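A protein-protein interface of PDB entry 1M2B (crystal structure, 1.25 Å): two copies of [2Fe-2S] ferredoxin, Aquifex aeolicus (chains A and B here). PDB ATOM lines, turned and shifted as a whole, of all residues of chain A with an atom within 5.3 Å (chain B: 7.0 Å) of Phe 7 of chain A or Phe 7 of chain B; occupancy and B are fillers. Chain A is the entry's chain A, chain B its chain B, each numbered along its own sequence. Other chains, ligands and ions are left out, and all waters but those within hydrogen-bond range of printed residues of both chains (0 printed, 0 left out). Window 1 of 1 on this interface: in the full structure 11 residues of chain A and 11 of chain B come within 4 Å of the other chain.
A ring nitrogen (ND1) of His 5 of chain A lies within hydrogen-bond range of the side-chain hydroxyl of Tyr 68 of chain B, 3.3 Å away. OH of Tyr 68 of chain A is in hydrogen-bond range of ND1 of His 5 of chain B.
The backbone NH (N) of His 5 of chain A lies within hydrogen-bond range of the backbone carbonyl oxygen (O) of Tyr 68 of chain A (2.9 Å). The backbone NH (N) of Tyr 68 of chain B is in hydrogen-bond range of the backbone carbonyl oxygen (O) of His 5 of chain B, 2.9 Å away. The backbone carbonyl oxygen of Val 6 of chain B lies within hydrogen-bond range of the backbone NH of Thr 51 of chain B. The backbone NH (N) of Phe 7 of chain B is in hydrogen-bond range of the backbone carbonyl oxygen (O) of Val 66 of chain B. O of Thr 51 of chain B sits at hydrogen-bond distance from N of Val 8 of chain B. The backbone NH of Thr 53 of chain B lies within hydrogen-bond range of the backbone carbonyl oxygen of Val 8 of chain B (2.9 Å).
Phe 7 of chain B touches Phe 7 of chain A. Phe 7 of chain A touches Tyr 68 of chain B. Thr 51 of chain A touches Thr 53 of chain B. Gly 54 of chain B touches Thr 51 of chain A. Thr 51 of chain A touches Met 56 of chain B. Thr 53 of chain A touches Thr 51 of chain B. Pro 52 of chain B touches Thr 53 of chain A. Met 56 of chain A touches His 5 of chain B (SD to CE1, 3.7 Å). Met 56 of chain A touches Thr 51 of chain B (CG to CG2, 3.7 Å). Tyr 68 of chain B touches Tyr 68 of chain A.
Phe 7 of chain A touches just these residues of chain B: Phe 7 and Tyr 68. Phe 7 of chain B touches just these residues of chain A: Phe 7 (3.4 Å) and Tyr 68 (3.7 Å). Of the printed residues of chain A, Trp 73 of chain B touches His 5. Of the printed residues of chain B, Thr 53 of chain A touches Thr 51 and Pro 52. Of the printed residues of chain B, Thr 51 of chain A touches Thr 53 (3.7 Å), Gly 54 (3.8 Å) and Met 56 (3.7 Å). The nearest residue of chain B that does not touch Phe 7 of chain A is Met 56 of chain B (4.1 Å). The nearest residue of chain A that does not touch Phe 7 of chain B is Met 56 of chain A (4.2 Å).
Of the 13 printed residues of chain A, 6 touch a printed residue of chain B. Hydrophobic or aromatic side chains of chain A within 4 Å of the printed part of chain B: His 5, Phe 7, Met 56 and Tyr 68. Along chain B the printed residues that touch a printed residue of chain A span positions 5 to 73. Among the printed residues, 15 pairs touch across the chains.
His 5 of chain A touches Met 56 of chain B, and with the chains exchanged Met 56 of chain A touches His 5 of chain B. His 5 of chain A touches Tyr 68 of chain B, and with the chains exchanged Tyr 68 of chain A touches His 5 of chain B. Thr 51 of chain A touches Thr 53 of chain B, and with the chains exchanged Thr 53 of chain A touches Thr 51 of chain B. Thr 51 of chain A touches Met 56 of chain B, and with the chains exchanged Met 56 of chain A touches Thr 51 of chain B. Positions printed for both chains: 5, 6, 7, 8, 9, 51, 53, 56, 64, 65, 66, 67 and 68.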
ATOM      1  N   HIS A   5      -6.735 -14.807  13.462  1.00  0.00           N
ATOM      2  CA  HIS A   5      -6.871 -14.234  14.803  1.00  0.00           C
ATOM      3  C   HIS A   5      -7.036 -12.734  14.649  1.00  0.00           C
ATOM      4  O   HIS A   5      -6.128 -12.075  14.165  1.00  0.00           O
ATOM      5  CB  HIS A   5      -5.647 -14.602  15.623  1.00  0.00           C
ATOM      6  CG  HIS A   5      -5.880 -14.525  17.099  1.00  0.00           C
ATOM      7  ND1 HIS A   5      -5.212 -15.063  18.108  1.00  0.00           N
ATOM      8  CD2 HIS A   5      -6.829 -13.905  17.830  1.00  0.00           C
ATOM      9  CE1 HIS A   5      -5.525 -14.934  19.312  1.00  0.00           C
ATOM     10  NE2 HIS A   5      -6.593 -14.164  19.164  1.00  0.00           N
ATOM     11  N   VAL A   6      -8.219 -12.249  15.030  1.00  0.00           N
ATOM     12  CA  VAL A   6      -8.590 -10.836  14.927  1.00  0.00           C
ATOM     13  C   VAL A   6      -8.496 -10.184  16.299  1.00  0.00           C
ATOM     14  O   VAL A   6      -9.119 -10.712  17.221  1.00  0.00           O
ATOM     15  CB  VAL A   6      -9.999 -10.734  14.376  1.00  0.00           C
ATOM     16  CG1 VAL A   6     -10.390  -9.276  14.152  1.00  0.00           C
ATOM     17  CG2 VAL A   6     -10.131 -11.452  13.028  1.00  0.00           C
ATOM     18  N   PHE A   7      -7.744  -9.129  16.398  1.00  0.00           N
ATOM     19  CA  PHE A   7      -7.591  -8.369  17.588  1.00  0.00           C
ATOM     20  C   PHE A   7      -8.251  -6.986  17.417  1.00  0.00           C
ATOM     21  O   PHE A   7      -7.918  -6.245  16.502  1.00  0.00           O
ATOM     22  CB  PHE A   7      -6.141  -8.189  17.955  1.00  0.00           C
ATOM     23  CG  PHE A   7      -5.431  -9.490  18.292  1.00  0.00           C
ATOM     24  CD1 PHE A   7      -4.784 -10.255  17.341  1.00  0.00           C
ATOM     25  CD2 PHE A   7      -5.449  -9.942  19.614  1.00  0.00           C
ATOM     26  CE1 PHE A   7      -4.172 -11.441  17.685  1.00  0.00           C
ATOM     27  CE2 PHE A   7      -4.817 -11.119  19.952  1.00  0.00           C
ATOM     28  CZ  PHE A   7      -4.163 -11.845  18.980  1.00  0.00           C
ATOM     29  N   VAL A   8      -9.173  -6.675  18.323  1.00  0.00           N
ATOM     30  CA  VAL A   8      -9.910  -5.389  18.294  1.00  0.00           C
ATOM     31  C   VAL A   8      -9.561  -4.637  19.545  1.00  0.00           C
ATOM     32  O   VAL A   8      -9.804  -5.084  20.679  1.00  0.00           O
ATOM     33  CB  VAL A   8     -11.423  -5.616  18.214  1.00  0.00           C
ATOM     34  CG1 VAL A   8     -12.184  -4.270  18.098  1.00  0.00           C
ATOM     35  CG2 VAL A   8     -11.788  -6.498  17.029  1.00  0.00           C
ATOM     36  N   CYS A   9      -8.976  -3.454  19.361  1.00  0.00           N
ATOM     37  CA  CYS A   9      -8.713  -2.593  20.511  1.00  0.00           C
ATOM     38  C   CYS A   9     -10.017  -2.077  21.079  1.00  0.00           C
ATOM     39  O   CYS A   9     -10.787  -1.472  20.351  1.00  0.00           O
ATOM     40  CB  CYS A   9      -7.798  -1.437  20.096  1.00  0.00           C
ATOM     41  SG  CYS A   9      -7.529  -0.317  21.521  1.00  0.00           S
ATOM     42  N   THR A  51     -10.445 -11.377  19.599  1.00  0.00           N
ATOM     43  CA  THR A  51      -9.907 -11.063  20.915  1.00  0.00           C
ATOM     44  C   THR A  51      -9.908  -9.557  21.163  1.00  0.00           C
ATOM     45  O   THR A  51      -9.355  -8.820  20.336  1.00  0.00           O
ATOM     46  CB  THR A  51      -8.465 -11.591  21.056  1.00  0.00           C
ATOM     47  OG1 THR A  51      -8.444 -12.997  20.889  1.00  0.00           O
ATOM     48  CG2 THR A  51      -7.887 -11.257  22.430  1.00  0.00           C
ATOM     49  N   THR A  53      -8.598  -6.162  23.038  1.00  0.00           N
ATOM     50  CA  THR A  53      -7.298  -5.772  23.547  1.00  0.00           C
ATOM     51  C   THR A  53      -7.290  -4.375  24.186  1.00  0.00           C
ATOM     52  O   THR A  53      -8.191  -3.567  23.955  1.00  0.00           O
ATOM     53  CB  THR A  53      -6.195  -5.795  22.457  1.00  0.00           C
ATOM     54  OG1 THR A  53      -6.362  -4.654  21.607  1.00  0.00           O
ATOM     55  CG2 THR A  53      -6.282  -7.033  21.604  1.00  0.00           C
ATOM     56  N   MET A  56      -3.135  -0.664  21.123  1.00  0.00           N
ATOM     57  CA  MET A  56      -2.068  -1.102  20.234  1.00  0.00           C
ATOM     58  C   MET A  56      -1.284   0.009  19.595  1.00  0.00           C
ATOM     59  O   MET A  56      -0.581  -0.066  18.615  1.00  0.00           O
ATOM     60  CB  MET A  56      -2.632  -2.045  19.158  1.00  0.00           C
ATOM     61  CG  MET A  56      -3.019  -3.385  19.820  1.00  0.00           C
ATOM     62  SD  MET A  56      -3.580  -4.646  18.662  1.00  0.00           S
ATOM     63  CE  MET A  56      -5.233  -4.043  18.324  1.00  0.00           C
ATOM     64  N   VAL A  64      -8.835   0.489  15.825  1.00  0.00           N
ATOM     65  CA  VAL A  64      -7.762  -0.340  15.310  1.00  0.00           C
ATOM     66  C   VAL A  64      -8.102  -1.834  15.417  1.00  0.00           C
ATOM     67  O   VAL A  64      -8.504  -2.301  16.489  1.00  0.00           O
ATOM     68  CB  VAL A  64      -6.424  -0.036  16.044  1.00  0.00           C
ATOM     69  CG1 VAL A  64      -5.340  -0.971  15.558  1.00  0.00           C
ATOM     70  CG2 VAL A  64      -6.014   1.424  15.862  1.00  0.00           C
ATOM     71  N   VAL A  65      -7.962  -2.545  14.319  1.00  0.00           N
ATOM     72  CA  VAL A  65      -8.219  -3.971  14.230  1.00  0.00           C
ATOM     73  C   VAL A  65      -7.022  -4.610  13.527  1.00  0.00           C
ATOM     74  O   VAL A  65      -6.645  -4.129  12.457  1.00  0.00           O
ATOM     75  CB  VAL A  65      -9.518  -4.277  13.463  1.00  0.00           C
ATOM     76  CG1 VAL A  65      -9.708  -5.779  13.316  1.00  0.00           C
ATOM     77  CG2 VAL A  65     -10.756  -3.628  14.089  1.00  0.00           C
ATOM     78  N   VAL A  66      -6.449  -5.655  14.119  1.00  0.00           N
ATOM     79  CA  VAL A  66      -5.283  -6.309  13.515  1.00  0.00           C
ATOM     80  C   VAL A  66      -5.609  -7.784  13.267  1.00  0.00           C
ATOM     81  O   VAL A  66      -6.167  -8.437  14.139  1.00  0.00           O
ATOM     82  CB  VAL A  66      -4.034  -6.141  14.387  1.00  0.00           C
ATOM     83  CG1 VAL A  66      -2.830  -6.768  13.648  1.00  0.00           C
ATOM     84  CG2 VAL A  66      -3.851  -4.666  14.814  1.00  0.00           C
ATOM     85  N   VAL A  67      -5.262  -8.259  12.095  1.00  0.00           N
ATOM     86  CA  VAL A  67      -5.484  -9.649  11.699  1.00  0.00           C
ATOM     87  C   VAL A  67      -4.164 -10.379  11.549  1.00  0.00           C
ATOM     88  O   VAL A  67      -3.339  -9.996  10.714  1.00  0.00           O
ATOM     89  CB  VAL A  67      -6.307  -9.736  10.398  1.00  0.00           C
ATOM     90  CG1 VAL A  67      -6.584 -11.181  10.022  1.00  0.00           C
ATOM     91  CG2 VAL A  67      -7.601  -8.945  10.517  1.00  0.00           C
ATOM     92  N   TYR A  68      -4.018 -11.469  12.295  1.00  0.00           N
ATOM     93  CA  TYR A  68      -2.843 -12.298  12.261  1.00  0.00           C
ATOM     94  C   TYR A  68      -3.253 -13.691  11.794  1.00  0.00           C
ATOM     95  O   TYR A  68      -4.408 -14.087  11.958  1.00  0.00           O
ATOM     96  CB  TYR A  68      -2.143 -12.360  13.634  1.00  0.00           C
ATOM     97  CG  TYR A  68      -1.312 -11.116  13.902  1.00  0.00           C
ATOM     98  CD1 TYR A  68      -1.586 -10.266  14.964  1.00  0.00           C
ATOM     99  CD2 TYR A  68      -0.279 -10.756  13.119  1.00  0.00           C
ATOM    100  CE1 TYR A  68      -0.817  -9.124  15.199  1.00  0.00           C
ATOM    101  CE2 TYR A  68       0.515  -9.648  13.288  1.00  0.00           C
ATOM    102  CZ  TYR A  68       0.223  -8.837  14.363  1.00  0.00           C
ATOM    103  OH  TYR A  68       1.062  -7.836  14.339  1.00  0.00           O
ATOM    104  N   HIS B   5       4.899  -9.267  17.685  1.00  0.00           N
ATOM    105  CA  HIS B   5       3.760  -8.723  18.394  1.00  0.00           C
ATOM    106  C   HIS B   5       3.390  -9.794  19.441  1.00  0.00           C
ATOM    107  O   HIS B   5       2.995 -10.909  19.089  1.00  0.00           O
ATOM    108  CB  HIS B   5       2.596  -8.409  17.449  1.00  0.00           C
ATOM    109  CG  HIS B   5       1.587  -7.454  18.000  1.00  0.00           C
ATOM    110  ND1 HIS B   5       0.655  -6.667  17.398  1.00  0.00           N
ATOM    111  CD2 HIS B   5       1.289  -7.080  19.287  1.00  0.00           C
ATOM    112  CE1 HIS B   5      -0.157  -5.914  17.980  1.00  0.00           C
ATOM    113  NE2 HIS B   5       0.268  -6.181  19.221  1.00  0.00           N
ATOM    114  N   VAL B   6       3.542  -9.441  20.699  1.00  0.00           N
ATOM    115  CA  VAL B   6       3.312 -10.334  21.816  1.00  0.00           C
ATOM    116  C   VAL B   6       2.018  -9.931  22.518  1.00  0.00           C
ATOM    117  O   VAL B   6       1.861  -8.766  22.892  1.00  0.00           O
ATOM    118  CB  VAL B   6       4.439 -10.232  22.834  1.00  0.00           C
ATOM    119  CG1 VAL B   6       4.250 -11.192  23.966  1.00  0.00           C
ATOM    120  CG2 VAL B   6       5.810 -10.485  22.187  1.00  0.00           C
ATOM    121  N   PHE B   7       1.134 -10.905  22.647  1.00  0.00           N
ATOM    122  CA  PHE B   7      -0.184 -10.719  23.256  1.00  0.00           C
ATOM    123  C   PHE B   7      -0.200 -11.459  24.576  1.00  0.00           C
ATOM    124  O   PHE B   7       0.068 -12.670  24.598  1.00  0.00           O
ATOM    125  CB  PHE B   7      -1.326 -11.213  22.370  1.00  0.00           C
ATOM    126  CG  PHE B   7      -1.455 -10.358  21.120  1.00  0.00           C
ATOM    127  CD1 PHE B   7      -0.791 -10.683  19.955  1.00  0.00           C
ATOM    128  CD2 PHE B   7      -2.234  -9.229  21.149  1.00  0.00           C
ATOM    129  CE1 PHE B   7      -0.908  -9.884  18.833  1.00  0.00           C
ATOM    130  CE2 PHE B   7      -2.390  -8.453  20.022  1.00  0.00           C
ATOM    131  CZ  PHE B   7      -1.751  -8.771  18.840  1.00  0.00           C
ATOM    132  N   VAL B   8      -0.491 -10.790  25.648  1.00  0.00           N
ATOM    133  CA  VAL B   8      -0.513 -11.374  26.992  1.00  0.00           C
ATOM    134  C   VAL B   8      -1.953 -11.269  27.505  1.00  0.00           C
ATOM    135  O   VAL B   8      -2.463 -10.165  27.668  1.00  0.00           O
ATOM    136  CB  VAL B   8       0.444 -10.691  27.959  1.00  0.00           C
ATOM    137  CG1 VAL B   8       0.388 -11.379  29.345  1.00  0.00           C
ATOM    138  CG2 VAL B   8       1.856 -10.665  27.392  1.00  0.00           C
ATOM    139  N   CYS B   9      -2.588 -12.427  27.793  1.00  0.00           N
ATOM    140  CA  CYS B   9      -3.915 -12.358  28.363  1.00  0.00           C
ATOM    141  C   CYS B   9      -3.833 -11.824  29.794  1.00  0.00           C
ATOM    142  O   CYS B   9      -3.104 -12.378  30.635  1.00  0.00           O
ATOM    143  CB  CYS B   9      -4.551 -13.751  28.362  1.00  0.00           C
ATOM    144  SG  CYS B   9      -6.177 -13.721  29.160  1.00  0.00           S
ATOM    145  N   PHE B  31       2.756  -9.675  31.955  1.00  0.00           N
ATOM    146  CA  PHE B  31       2.625  -8.506  31.066  1.00  0.00           C
ATOM    147  C   PHE B  31       3.594  -7.411  31.451  1.00  0.00           C
ATOM    148  O   PHE B  31       4.294  -6.830  30.621  1.00  0.00           O
ATOM    149  CB  PHE B  31       1.155  -8.023  31.116  1.00  0.00           C
ATOM    150  CG  PHE B  31       0.928  -6.730  30.360  1.00  0.00           C
ATOM    151  CD1 PHE B  31       1.038  -6.676  28.990  1.00  0.00           C
ATOM    152  CD2 PHE B  31       0.627  -5.569  31.032  1.00  0.00           C
ATOM    153  CE1 PHE B  31       0.883  -5.476  28.269  1.00  0.00           C
ATOM    154  CE2 PHE B  31       0.446  -4.371  30.366  1.00  0.00           C
ATOM    155  CZ  PHE B  31       0.576  -4.329  28.988  1.00  0.00           C
ATOM    156  N   PHE B  34       7.164  -8.230  30.449  1.00  0.00           N
ATOM    157  CA  PHE B  34       7.416  -7.974  29.025  1.00  0.00           C
ATOM    158  C   PHE B  34       7.543  -6.483  28.742  1.00  0.00           C
ATOM    159  O   PHE B  34       8.423  -6.043  28.002  1.00  0.00           O
ATOM    160  CB  PHE B  34       6.307  -8.547  28.125  1.00  0.00           C
ATOM    161  CG  PHE B  34       6.499 -10.012  27.771  1.00  0.00           C
ATOM    162  CD1 PHE B  34       5.694 -11.000  28.310  1.00  0.00           C
ATOM    163  CD2 PHE B  34       7.479 -10.420  26.865  1.00  0.00           C
ATOM    164  CE1 PHE B  34       5.822 -12.323  27.949  1.00  0.00           C
ATOM    165  CE2 PHE B  34       7.645 -11.732  26.466  1.00  0.00           C
ATOM    166  CZ  PHE B  34       6.800 -12.687  27.027  1.00  0.00           C
ATOM    167  N   VAL B  49       6.102  -5.157  19.972  1.00  0.00           N
ATOM    168  CA  VAL B  49       4.904  -4.580  20.577  1.00  0.00           C
ATOM    169  C   VAL B  49       4.366  -5.596  21.604  1.00  0.00           C
ATOM    170  O   VAL B  49       4.325  -6.776  21.251  1.00  0.00           O
ATOM    171  CB  VAL B  49       3.799  -4.170  19.570  1.00  0.00           C
ATOM    172  CG1 VAL B  49       2.522  -3.668  20.255  1.00  0.00           C
ATOM    173  CG2 VAL B  49       4.369  -3.120  18.631  1.00  0.00           C
ATOM    174  N   ILE B  50       3.995  -5.146  22.777  1.00  0.00           N
ATOM    175  CA  ILE B  50       3.405  -5.943  23.843  1.00  0.00           C
ATOM    176  C   ILE B  50       1.996  -5.397  24.090  1.00  0.00           C
ATOM    177  O   ILE B  50       1.817  -4.232  24.431  1.00  0.00           O
ATOM    178  CB  ILE B  50       4.202  -5.892  25.159  1.00  0.00           C
ATOM    179  CG1 ILE B  50       5.703  -6.083  25.005  1.00  0.00           C
ATOM    180  CG2 ILE B  50       3.589  -6.890  26.148  1.00  0.00           C
ATOM    181  CD1 ILE B  50       6.118  -7.443  24.403  1.00  0.00           C
ATOM    182  N   THR B  51       1.017  -6.284  23.928  1.00  0.00           N
ATOM    183  CA  THR B  51      -0.394  -5.891  24.017  1.00  0.00           C
ATOM    184  C   THR B  51      -1.135  -6.748  25.049  1.00  0.00           C
ATOM    185  O   THR B  51      -1.066  -7.981  24.948  1.00  0.00           O
ATOM    186  CB  THR B  51      -1.077  -6.032  22.661  1.00  0.00           C
ATOM    187  OG1 THR B  51      -0.396  -5.235  21.694  1.00  0.00           O
ATOM    188  CG2 THR B  51      -2.533  -5.595  22.698  1.00  0.00           C
ATOM    189  N   PRO B  52      -1.825  -6.135  25.999  1.00  0.00           N
ATOM    190  CA  PRO B  52      -2.655  -6.907  26.951  1.00  0.00           C
ATOM    191  C   PRO B  52      -4.011  -7.200  26.357  1.00  0.00           C
ATOM    192  O   PRO B  52      -4.558  -6.381  25.616  1.00  0.00           O
ATOM    193  CB  PRO B  52      -2.738  -5.944  28.134  1.00  0.00           C
ATOM    194  CG  PRO B  52      -2.788  -4.586  27.484  1.00  0.00           C
ATOM    195  CD  PRO B  52      -1.917  -4.691  26.278  1.00  0.00           C
ATOM    196  N   THR B  53      -4.551  -8.409  26.659  1.00  0.00           N
ATOM    197  CA  THR B  53      -5.774  -8.855  26.033  1.00  0.00           C
ATOM    198  C   THR B  53      -6.782  -9.384  27.061  1.00  0.00           C
ATOM    199  O   THR B  53      -6.423  -9.730  28.181  1.00  0.00           O
ATOM    200  CB  THR B  53      -5.577  -9.937  24.967  1.00  0.00           C
ATOM    201  OG1 THR B  53      -5.244 -11.196  25.582  1.00  0.00           O
ATOM    202  CG2 THR B  53      -4.402  -9.596  24.064  1.00  0.00           C
ATOM    203  N   GLY B  54      -8.022  -9.496  26.576  1.00  0.00           N
ATOM    204  CA  GLY B  54      -8.979 -10.363  27.236  1.00  0.00           C
ATOM    205  C   GLY B  54      -8.709 -11.814  26.855  1.00  0.00           C
ATOM    206  O   GLY B  54      -7.776 -12.169  26.107  1.00  0.00           O
ATOM    207  N   MET B  56      -8.137 -15.405  25.532  1.00  0.00           N
ATOM    208  CA  MET B  56      -7.921 -16.011  24.233  1.00  0.00           C
ATOM    209  C   MET B  56      -8.248 -17.487  24.193  1.00  0.00           C
ATOM    210  O   MET B  56      -7.845 -18.299  23.376  1.00  0.00           O
ATOM    211  CB  MET B  56      -6.445 -15.829  23.806  1.00  0.00           C
ATOM    212  CG  MET B  56      -6.164 -14.389  23.480  1.00  0.00           C
ATOM    213  SD  MET B  56      -4.523 -14.019  22.865  1.00  0.00           S
ATOM    214  CE  MET B  56      -3.590 -13.979  24.391  1.00  0.00           C
ATOM    215  N   VAL B  64      -1.430 -17.306  29.401  1.00  0.00           N
ATOM    216  CA  VAL B  64      -1.343 -17.509  27.959  1.00  0.00           C
ATOM    217  C   VAL B  64      -0.674 -16.299  27.312  1.00  0.00           C
ATOM    218  O   VAL B  64      -1.090 -15.157  27.537  1.00  0.00           O
ATOM    219  CB  VAL B  64      -2.718 -17.762  27.351  1.00  0.00           C
ATOM    220  CG1 VAL B  64      -2.607 -17.884  25.837  1.00  0.00           C
ATOM    221  CG2 VAL B  64      -3.355 -18.990  27.985  1.00  0.00           C
ATOM    222  N   VAL B  65       0.346 -16.574  26.517  1.00  0.00           N
ATOM    223  CA  VAL B  65       1.072 -15.563  25.763  1.00  0.00           C
ATOM    224  C   VAL B  65       1.179 -16.016  24.308  1.00  0.00           C
ATOM    225  O   VAL B  65       1.554 -17.152  24.081  1.00  0.00           O
ATOM    226  CB  VAL B  65       2.477 -15.346  26.374  1.00  0.00           C
ATOM    227  CG1 VAL B  65       3.299 -14.362  25.518  1.00  0.00           C
ATOM    228  CG2 VAL B  65       2.402 -14.919  27.825  1.00  0.00           C
ATOM    229  N   VAL B  66       0.801 -15.160  23.360  1.00  0.00           N
ATOM    230  CA  VAL B  66       0.819 -15.536  21.951  1.00  0.00           C
ATOM    231  C   VAL B  66       1.734 -14.553  21.193  1.00  0.00           C
ATOM    232  O   VAL B  66       1.628 -13.347  21.380  1.00  0.00           O
ATOM    233  CB  VAL B  66      -0.590 -15.558  21.334  1.00  0.00           C
ATOM    234  CG1 VAL B  66      -0.548 -16.071  19.916  1.00  0.00           C
ATOM    235  CG2 VAL B  66      -1.501 -16.390  22.223  1.00  0.00           C
ATOM    236  N   VAL B  67       2.632 -15.099  20.370  1.00  0.00           N
ATOM    237  CA  VAL B  67       3.548 -14.328  19.604  1.00  0.00           C
ATOM    238  C   VAL B  67       3.208 -14.446  18.113  1.00  0.00           C
ATOM    239  O   VAL B  67       3.232 -15.540  17.547  1.00  0.00           O
ATOM    240  CB  VAL B  67       5.009 -14.766  19.840  1.00  0.00           C
ATOM    241  CG1 VAL B  67       5.970 -13.909  19.043  1.00  0.00           C
ATOM    242  CG2 VAL B  67       5.317 -14.750  21.330  1.00  0.00           C
ATOM    243  N   TYR B  68       2.924 -13.303  17.509  1.00  0.00           N
ATOM    244  CA  TYR B  68       2.644 -13.156  16.091  1.00  0.00           C
ATOM    245  C   TYR B  68       3.764 -12.377  15.392  1.00  0.00           C
ATOM    246  O   TYR B  68       4.477 -11.624  16.077  1.00  0.00           O
ATOM    247  CB  TYR B  68       1.267 -12.537  15.865  1.00  0.00           C
ATOM    248  CG  TYR B  68       0.167 -13.540  16.089  1.00  0.00           C
ATOM    249  CD1 TYR B  68      -0.802 -13.338  17.076  1.00  0.00           C
ATOM    250  CD2 TYR B  68       0.050 -14.668  15.322  1.00  0.00           C
ATOM    251  CE1 TYR B  68      -1.816 -14.267  17.248  1.00  0.00           C
ATOM    252  CE2 TYR B  68      -0.939 -15.616  15.493  1.00  0.00           C
ATOM    253  CZ  TYR B  68      -1.904 -15.399  16.473  1.00  0.00           C
ATOM    254  OH  TYR B  68      -2.725 -16.449  16.477  1.00  0.00           O
ATOM    255  N   TRP B  73       1.905 -20.094  20.597  1.00  0.00           N
ATOM    256  CA  TRP B  73       1.119 -20.027  21.809  1.00  0.00           C
ATOM    257  C   TRP B  73       1.912 -20.667  22.951  1.00  0.00           C
ATOM    258  O   TRP B  73       2.297 -21.831  22.839  1.00  0.00           O
ATOM    259  CB  TRP B  73      -0.257 -20.719  21.731  1.00  0.00           C
ATOM    260  CG  TRP B  73      -1.188 -20.084  20.717  1.00  0.00           C
ATOM    261  CD1 TRP B  73      -0.998 -19.928  19.375  1.00  0.00           C
ATOM    262  CD2 TRP B  73      -2.466 -19.523  20.995  1.00  0.00           C
ATOM    263  NE1 TRP B  73      -2.091 -19.302  18.806  1.00  0.00           N
ATOM    264  CE2 TRP B  73      -2.998 -19.048  19.774  1.00  0.00           C
ATOM    265  CE3 TRP B  73      -3.236 -19.385  22.125  1.00  0.00           C
ATOM    266  CZ2 TRP B  73      -4.240 -18.441  19.698  1.00  0.00           C
ATOM    267  CZ3 TRP B  73      -4.467 -18.786  22.083  1.00  0.00           C
ATOM    268  CH2 TRP B  73      -4.967 -18.314  20.868  1.00  0.00           C
